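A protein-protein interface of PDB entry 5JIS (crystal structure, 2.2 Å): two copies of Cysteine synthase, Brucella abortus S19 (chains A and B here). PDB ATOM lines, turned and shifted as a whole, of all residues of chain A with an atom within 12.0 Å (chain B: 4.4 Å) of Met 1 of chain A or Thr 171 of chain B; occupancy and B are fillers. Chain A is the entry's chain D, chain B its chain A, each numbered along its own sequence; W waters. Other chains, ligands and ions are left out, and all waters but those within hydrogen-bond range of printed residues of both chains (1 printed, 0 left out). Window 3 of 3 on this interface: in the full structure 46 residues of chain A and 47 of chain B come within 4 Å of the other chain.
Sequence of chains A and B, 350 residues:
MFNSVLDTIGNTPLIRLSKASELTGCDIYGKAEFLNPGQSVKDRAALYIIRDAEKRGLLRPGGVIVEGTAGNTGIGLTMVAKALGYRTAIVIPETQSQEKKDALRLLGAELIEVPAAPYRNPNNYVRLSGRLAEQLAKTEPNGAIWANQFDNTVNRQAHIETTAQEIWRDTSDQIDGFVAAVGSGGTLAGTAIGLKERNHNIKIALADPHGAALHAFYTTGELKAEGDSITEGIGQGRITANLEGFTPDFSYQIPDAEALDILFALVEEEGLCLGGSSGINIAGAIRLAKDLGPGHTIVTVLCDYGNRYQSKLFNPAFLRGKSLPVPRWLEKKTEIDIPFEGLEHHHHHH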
ATOM      1  N   MET A   1     -14.764   4.656  -5.345  1.00  0.00           N
ATOM      2  CA  MET A   1     -15.979   5.511  -5.108  1.00  0.00           C
ATOM      3  C   MET A   1     -16.030   6.019  -3.662  1.00  0.00           C
ATOM      4  O   MET A   1     -16.285   5.239  -2.741  1.00  0.00           O
ATOM      5  CB  MET A   1     -17.270   4.746  -5.446  1.00  0.00           C
ATOM      6  CG  MET A   1     -17.553   4.639  -6.938  1.00  0.00           C
ATOM      7  SD  MET A   1     -18.953   3.586  -7.391  1.00  0.00           S
ATOM      8  CE  MET A   1     -18.485   1.981  -6.736  1.00  0.00           C
ATOM      9  N   PHE A   2     -15.792   7.324  -3.480  1.00  0.00           N
ATOM     10  CA  PHE A   2     -15.742   7.964  -2.153  1.00  0.00           C
ATOM     11  C   PHE A   2     -16.658   9.205  -2.069  1.00  0.00           C
ATOM     12  O   PHE A   2     -16.645  10.051  -2.965  1.00  0.00           O
ATOM     13  CB  PHE A   2     -14.293   8.376  -1.820  1.00  0.00           C
ATOM     14  CG  PHE A   2     -13.376   7.231  -1.386  1.00  0.00           C
ATOM     15  CD1 PHE A   2     -13.802   6.233  -0.487  1.00  0.00           C
ATOM     16  CD2 PHE A   2     -12.051   7.184  -1.843  1.00  0.00           C
ATOM     17  CE1 PHE A   2     -12.938   5.217  -0.084  1.00  0.00           C
ATOM     18  CE2 PHE A   2     -11.186   6.167  -1.441  1.00  0.00           C
ATOM     19  CZ  PHE A   2     -11.632   5.184  -0.562  1.00  0.00           C
ATOM     20  N   ASN A   3     -17.410   9.319  -0.968  1.00  0.00           N
ATOM     21  CA  ASN A   3     -18.452  10.360  -0.782  1.00  0.00           C
ATOM     22  C   ASN A   3     -17.991  11.806  -0.602  1.00  0.00           C
ATOM     23  O   ASN A   3     -18.779  12.729  -0.824  1.00  0.00           O
ATOM     24  CB  ASN A   3     -19.350  10.007   0.410  1.00  0.00           C
ATOM     25  CG  ASN A   3     -20.270   8.846   0.115  1.00  0.00           C
ATOM     26  OD1 ASN A   3     -20.741   8.687  -1.011  1.00  0.00           O
ATOM     27  ND2 ASN A   3     -20.539   8.028   1.128  1.00  0.00           N
ATOM     28  N   SER A   4     -16.752  12.012  -0.160  1.00  0.00           N
ATOM     29  CA  SER A   4     -16.157  13.349  -0.174  1.00  0.00           C
ATOM     30  C   SER A   4     -14.630  13.273  -0.136  1.00  0.00           C
ATOM     31  O   SER A   4     -14.045  12.188  -0.014  1.00  0.00           O
ATOM     32  CB  SER A   4     -16.682  14.216   0.994  1.00  0.00           C
ATOM     33  OG  SER A   4     -15.966  14.000   2.198  1.00  0.00           O
ATOM     34  N   VAL A   5     -14.000  14.444  -0.232  1.00  0.00           N
ATOM     35  CA  VAL A   5     -12.555  14.554  -0.091  1.00  0.00           C
ATOM     36  C   VAL A   5     -12.066  13.918   1.217  1.00  0.00           C
ATOM     37  O   VAL A   5     -10.962  13.406   1.275  1.00  0.00           O
ATOM     38  CB  VAL A   5     -12.072  16.021  -0.236  1.00  0.00           C
ATOM     39  CG1 VAL A   5     -12.542  16.898   0.929  1.00  0.00           C
ATOM     40  CG2 VAL A   5     -10.559  16.076  -0.382  1.00  0.00           C
ATOM     41  N   LEU A   6     -12.910  13.927   2.247  1.00  0.00           N
ATOM     42  CA  LEU A   6     -12.583  13.333   3.552  1.00  0.00           C
ATOM     43  C   LEU A   6     -12.189  11.843   3.536  1.00  0.00           C
ATOM     44  O   LEU A   6     -11.367  11.419   4.346  1.00  0.00           O
ATOM     45  CB  LEU A   6     -13.731  13.562   4.537  1.00  0.00           C
ATOM     46  CG  LEU A   6     -14.132  15.030   4.794  1.00  0.00           C
ATOM     47  CD1 LEU A   6     -15.100  15.102   5.959  1.00  0.00           C
ATOM     48  CD2 LEU A   6     -12.933  15.928   5.058  1.00  0.00           C
ATOM     49  N   ASP A   7     -12.764  11.063   2.627  1.00  0.00           N
ATOM     50  CA  ASP A   7     -12.395   9.643   2.496  1.00  0.00           C
ATOM     51  C   ASP A   7     -11.014   9.415   1.870  1.00  0.00           C
ATOM     52  O   ASP A   7     -10.513   8.289   1.888  1.00  0.00           O
ATOM     53  CB  ASP A   7     -13.444   8.892   1.686  1.00  0.00           C
ATOM     54  CG  ASP A   7     -14.679   8.551   2.503  1.00  0.00           C
ATOM     55  OD1 ASP A   7     -14.537   7.894   3.558  1.00  0.00           O
ATOM     56  OD2 ASP A   7     -15.788   8.941   2.084  1.00  0.00           O
ATOM     57  N   THR A   8     -10.411  10.468   1.317  1.00  0.00           N
ATOM     58  CA  THR A   8      -9.042  10.401   0.786  1.00  0.00           C
ATOM     59  C   THR A   8      -8.009  10.775   1.845  1.00  0.00           C
ATOM     60  O   THR A   8      -6.820  10.706   1.570  1.00  0.00           O
ATOM     61  CB  THR A   8      -8.857  11.294  -0.471  1.00  0.00           C
ATOM     62  OG1 THR A   8      -8.830  12.684  -0.114  1.00  0.00           O
ATOM     63  CG2 THR A   8      -9.959  11.033  -1.491  1.00  0.00           C
ATOM     64  N   ILE A   9      -8.448  11.181   3.042  1.00  0.00           N
ATOM     65  CA  ILE A   9      -7.518  11.392   4.158  1.00  0.00           C
ATOM     66  C   ILE A   9      -6.994  10.036   4.645  1.00  0.00           C
ATOM     67  O   ILE A   9      -7.762   9.097   4.841  1.00  0.00           O
ATOM     68  CB  ILE A   9      -8.167  12.177   5.317  1.00  0.00           C
ATOM     69  CG1 ILE A   9      -8.425  13.616   4.874  1.00  0.00           C
ATOM     70  CG2 ILE A   9      -7.271  12.160   6.549  1.00  0.00           C
ATOM     71  CD1 ILE A   9      -9.320  14.411   5.799  1.00  0.00           C
ATOM     72  N   ASN A  11      -4.469   6.478   4.880  1.00  0.00           N
ATOM     73  CA  ASN A  11      -3.922   5.379   4.080  1.00  0.00           C
ATOM     74  C   ASN A  11      -2.823   5.828   3.127  1.00  0.00           C
ATOM     75  O   ASN A  11      -2.838   5.517   1.944  1.00  0.00           O
ATOM     76  CB  ASN A  11      -5.068   4.668   3.356  1.00  0.00           C
ATOM     77  CG  ASN A  11      -5.882   3.830   4.314  1.00  0.00           C
ATOM     78  OD1 ASN A  11      -5.339   2.932   4.967  1.00  0.00           O
ATOM     79  ND2 ASN A  11      -7.157   4.143   4.449  1.00  0.00           N
ATOM     80  N   LEU B  14     -11.520   8.356  -6.627  1.00  0.00           N
ATOM     81  CA  LEU B  14     -12.655   9.108  -7.148  1.00  0.00           C
ATOM     82  C   LEU B  14     -13.339   9.823  -5.991  1.00  0.00           C
ATOM     83  O   LEU B  14     -13.645   9.198  -4.973  1.00  0.00           O
ATOM     84  CB  LEU B  14     -13.634   8.154  -7.830  1.00  0.00           C
ATOM     85  CG  LEU B  14     -13.081   7.385  -9.038  1.00  0.00           C
ATOM     86  CD1 LEU B  14     -14.161   6.520  -9.663  1.00  0.00           C
ATOM     87  CD2 LEU B  14     -12.501   8.307 -10.098  1.00  0.00           C
ATOM     88  N   TYR B  29     -18.280  11.855 -10.292  1.00  0.00           N
ATOM     89  CA  TYR B  29     -17.021  11.754  -9.570  1.00  0.00           C
ATOM     90  C   TYR B  29     -15.919  12.488 -10.314  1.00  0.00           C
ATOM     91  O   TYR B  29     -15.861  12.476 -11.548  1.00  0.00           O
ATOM     92  CB  TYR B  29     -16.588  10.299  -9.435  1.00  0.00           C
ATOM     93  CG  TYR B  29     -17.545   9.466  -8.641  1.00  0.00           C
ATOM     94  CD1 TYR B  29     -17.428   9.373  -7.256  1.00  0.00           C
ATOM     95  CD2 TYR B  29     -18.582   8.781  -9.269  1.00  0.00           C
ATOM     96  CE1 TYR B  29     -18.330   8.618  -6.513  1.00  0.00           C
ATOM     97  CE2 TYR B  29     -19.479   8.023  -8.541  1.00  0.00           C
ATOM     98  CZ  TYR B  29     -19.349   7.947  -7.163  1.00  0.00           C
ATOM     99  OH  TYR B  29     -20.235   7.202  -6.444  1.00  0.00           O
ATOM    100  N   ILE B 167     -10.434   3.694 -13.253  1.00  0.00           N
ATOM    101  CA  ILE B 167     -11.801   4.204 -13.286  1.00  0.00           C
ATOM    102  C   ILE B 167     -12.803   3.058 -13.418  1.00  0.00           C
ATOM    103  O   ILE B 167     -13.794   3.004 -12.688  1.00  0.00           O
ATOM    104  CB  ILE B 167     -11.983   5.236 -14.425  1.00  0.00           C
ATOM    105  CG1 ILE B 167     -11.323   6.557 -14.043  1.00  0.00           C
ATOM    106  CG2 ILE B 167     -13.459   5.468 -14.727  1.00  0.00           C
ATOM    107  CD1 ILE B 167     -11.114   7.528 -15.195  1.00  0.00           C
ATOM    108  N   TRP B 168     -12.547   2.175 -14.374  1.00  0.00           N
ATOM    109  CA  TRP B 168     -13.370   0.983 -14.589  1.00  0.00           C
ATOM    110  C   TRP B 168     -13.430   0.143 -13.303  1.00  0.00           C
ATOM    111  O   TRP B 168     -14.514  -0.198 -12.829  1.00  0.00           O
ATOM    112  CB  TRP B 168     -12.821   0.177 -15.779  1.00  0.00           C
ATOM    113  CG  TRP B 168     -13.508  -1.118 -16.050  1.00  0.00           C
ATOM    114  CD1 TRP B 168     -13.035  -2.362 -15.763  1.00  0.00           C
ATOM    115  CD2 TRP B 168     -14.801  -1.304 -16.660  1.00  0.00           C
ATOM    116  NE1 TRP B 168     -13.952  -3.320 -16.161  1.00  0.00           N
ATOM    117  CE2 TRP B 168     -15.042  -2.698 -16.711  1.00  0.00           C
ATOM    118  CE3 TRP B 168     -15.778  -0.428 -17.167  1.00  0.00           C
ATOM    119  CZ2 TRP B 168     -16.215  -3.241 -17.258  1.00  0.00           C
ATOM    120  CZ3 TRP B 168     -16.947  -0.963 -17.702  1.00  0.00           C
ATOM    121  CH2 TRP B 168     -17.158  -2.363 -17.742  1.00  0.00           C
ATOM    122  N   ARG B 169     -12.262  -0.134 -12.726  1.00  0.00           N
ATOM    123  CA  ARG B 169     -12.156  -0.927 -11.500  1.00  0.00           C
ATOM    124  C   ARG B 169     -12.897  -0.271 -10.333  1.00  0.00           C
ATOM    125  O   ARG B 169     -13.700  -0.916  -9.675  1.00  0.00           O
ATOM    126  CB  ARG B 169     -10.681  -1.150 -11.135  1.00  0.00           C
ATOM    127  CG  ARG B 169     -10.420  -2.038  -9.910  1.00  0.00           C
ATOM    128  CD  ARG B 169      -8.973  -1.908  -9.419  1.00  0.00           C
ATOM    129  NE  ARG B 169      -8.661  -0.524  -9.054  1.00  0.00           N
ATOM    130  CZ  ARG B 169      -7.452   0.039  -9.019  1.00  0.00           C
ATOM    131  NH1 ARG B 169      -6.346  -0.647  -9.306  1.00  0.00           N
ATOM    132  NH2 ARG B 169      -7.347   1.321  -8.672  1.00  0.00           N
ATOM    133  N   ASP B 170     -12.632   1.008 -10.088  1.00  0.00           N
ATOM    134  CA  ASP B 170     -13.138   1.675  -8.885  1.00  0.00           C
ATOM    135  C   ASP B 170     -14.601   2.094  -8.966  1.00  0.00           C
ATOM    136  O   ASP B 170     -15.173   2.474  -7.942  1.00  0.00           O
ATOM    137  CB  ASP B 170     -12.266   2.888  -8.539  1.00  0.00           C
ATOM    138  CG  ASP B 170     -10.844   2.498  -8.177  1.00  0.00           C
ATOM    139  OD1 ASP B 170     -10.620   1.343  -7.777  1.00  0.00           O
ATOM    140  OD2 ASP B 170      -9.945   3.345  -8.300  1.00  0.00           O
ATOM    141  N   THR B 171     -15.185   2.069 -10.168  1.00  0.00           N
ATOM    142  CA  THR B 171     -16.631   2.222 -10.322  1.00  0.00           C
ATOM    143  C   THR B 171     -17.347   0.872 -10.402  1.00  0.00           C
ATOM    144  O   THR B 171     -18.550   0.849 -10.636  1.00  0.00           O
ATOM    145  CB  THR B 171     -17.008   3.049 -11.577  1.00  0.00           C
ATOM    146  OG1 THR B 171     -16.579   2.378 -12.765  1.00  0.00           O
ATOM    147  CG2 THR B 171     -16.437   4.455 -11.502  1.00  0.00           C
ATOM    148  N   SER B 172     -16.617  -0.238 -10.220  1.00  0.00           N
ATOM    149  CA  SER B 172     -17.163  -1.593 -10.331  1.00  0.00           C
ATOM    150  C   SER B 172     -17.914  -1.784 -11.663  1.00  0.00           C
ATOM    151  O   SER B 172     -19.001  -2.371 -11.696  1.00  0.00           O
ATOM    152  CB  SER B 172     -18.083  -1.903  -9.133  1.00  0.00           C
ATOM    153  OG  SER B 172     -17.373  -1.791  -7.908  1.00  0.00           O
ATOM    154  N   ASP B 173     -17.325  -1.268 -12.744  1.00  0.00           N
ATOM    155  CA  ASP B 173     -17.873  -1.393 -14.098  1.00  0.00           C
ATOM    156  C   ASP B 173     -19.139  -0.560 -14.366  1.00  0.00           C
ATOM    157  O   ASP B 173     -19.742  -0.737 -15.416  1.00  0.00           O
ATOM    158  CB  ASP B 173     -18.178  -2.875 -14.465  1.00  0.00           C
ATOM    159  CG  ASP B 173     -17.002  -3.828 -14.225  1.00  0.00           C
ATOM    160  OD1 ASP B 173     -15.976  -3.455 -13.647  1.00  0.00           O
ATOM    161  OD2 ASP B 173     -17.120  -4.988 -14.631  1.00  0.00           O
ATOM    162  N   GLN B 174     -19.540   0.341 -13.462  1.00  0.00           N
ATOM    163  CA  GLN B 174     -20.804   1.098 -13.627  1.00  0.00           C
ATOM    164  C   GLN B 174     -20.652   2.410 -14.387  1.00  0.00           C
ATOM    165  O   GLN B 174     -21.657   3.027 -14.739  1.00  0.00           O
ATOM    166  CB  GLN B 174     -21.460   1.385 -12.269  1.00  0.00           C
ATOM    167  CG  GLN B 174     -22.004   0.147 -11.568  1.00  0.00           C
ATOM    168  CD  GLN B 174     -22.313   0.371 -10.093  1.00  0.00           C
ATOM    169  OE1 GLN B 174     -22.384   1.505  -9.609  1.00  0.00           O
ATOM    170  NE2 GLN B 174     -22.510  -0.721  -9.370  1.00  0.00           N
ATOM    171  N   ILE B 175     -19.416   2.847 -14.637  1.00  0.00           N
ATOM    172  CA  ILE B 175     -19.180   4.108 -15.365  1.00  0.00           C
ATOM    173  C   ILE B 175     -19.889   4.176 -16.728  1.00  0.00           C
ATOM    174  O   ILE B 175     -19.712   3.308 -17.575  1.00  0.00           O
ATOM    175  CB  ILE B 175     -17.674   4.445 -15.539  1.00  0.00           C
ATOM    176  CG1 ILE B 175     -17.520   5.720 -16.382  1.00  0.00           C
ATOM    177  CG2 ILE B 175     -16.888   3.310 -16.193  1.00  0.00           C
ATOM    178  CD1 ILE B 175     -16.223   6.439 -16.190  1.00  0.00           C
ATOM    179  N   VAL B 299     -17.644  10.300 -14.840  1.00  0.00           N
ATOM    180  CA  VAL B 299     -16.342  10.578 -14.223  1.00  0.00           C
ATOM    181  C   VAL B 299     -15.611  11.638 -15.011  1.00  0.00           C
ATOM    182  O   VAL B 299     -15.647  11.642 -16.231  1.00  0.00           O
ATOM    183  CB  VAL B 299     -15.495   9.305 -14.061  1.00  0.00           C
ATOM    184  CG1 VAL B 299     -14.131   9.616 -13.457  1.00  0.00           C
ATOM    185  CG2 VAL B 299     -16.212   8.315 -13.160  1.00  0.00           C
HETATM  186  O   HOH W   1     -11.875   5.316  -5.805  1.00  0.00           O
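No position is printed for both chains. Of the 4 pairs that touch across the chains among the printed residues, none has its exchanged pair printed and touching as well.
NE of Arg 169 of chain B is in salt-bridge range of OD1 of Asp 170 of chain B, 3.0 Å away. OG1 of Thr 171 of chain B lies within hydrogen-bond range of N of Ile 175 of chain B (3.4 Å). OG1 of Thr 171 of chain B sits at hydrogen-bond distance from O of Ile 167 of chain B (2.9 Å). The side-chain hydroxyl (OG1) of Thr 171 of chain B lies within hydrogen-bond range of the backbone carbonyl oxygen (O) of Trp 168 of chain B (3.3 Å).
Printed residues of chain A within 4 Å of Thr 171 of chain B: Met 1. No residue of chain A comes within 4 Å of Ile 167 of chain B. Of chain A, only Met 1 comes within 4 Å of Asp 170 of chain B. No residue of chain A comes within 4 Å of Asp 173 of chain B. No residue of chain A comes within 4 Å of Gln 174 of chain B. No residue of chain A comes within 4 Å of Ile 175 of chain B. Of the printed residues of chain B, Phe 2 of chain A touches Leu 14 (3.2 Å). Of the printed residues of chain A, Tyr 29 of chain B touches Met 1 (3.7 Å). Asn 3 of chain A touches none of the printed residues of chain B. Thr 8 of chain A touches none of the printed residues of chain B. The nearest printed residue of chain A that does not touch Thr 171 of chain B is Phe 2 of chain A (8.5 Å). The nearest printed residue of chain B that does not touch Phe 2 of chain A is Tyr 29 of chain B (4.2 Å).
The backbone NH (N) of Phe 2 of chain A sits at hydrogen-bond distance from the backbone carbonyl oxygen (O) of Leu 14 of chain B (3.2 Å). O of Asp 170 of chain B sits close to N of Met 1 of chain A, 3.4 Å away.
Hydrophobic or aromatic side chains of chain B within 4 Å of the printed part of chain A: Tyr 29. Of the 10 printed residues of chain A, 2 touch a printed residue of chain B. Hydrophobic or aromatic side chains of chain A that line the printed part of chain B: Met 1 and Phe 2. Among the printed residues, 4 pairs touch across the chains. Among the printed residues, no Asp or Glu carboxylate lies within 4 Å of a Lys or Arg side-chain nitrogen of the other chain.
Among the printed residues, pairs that only touch across the chains: Met 1 of chain A with Tyr 29 of chain B and Met 1 of chain A with Thr 171 of chain B.
Water W1 lies within hydrogen-bond range of N of Met 1 of chain A (3.0 Å) and N of Leu 14 of chain B (3.2 Å).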
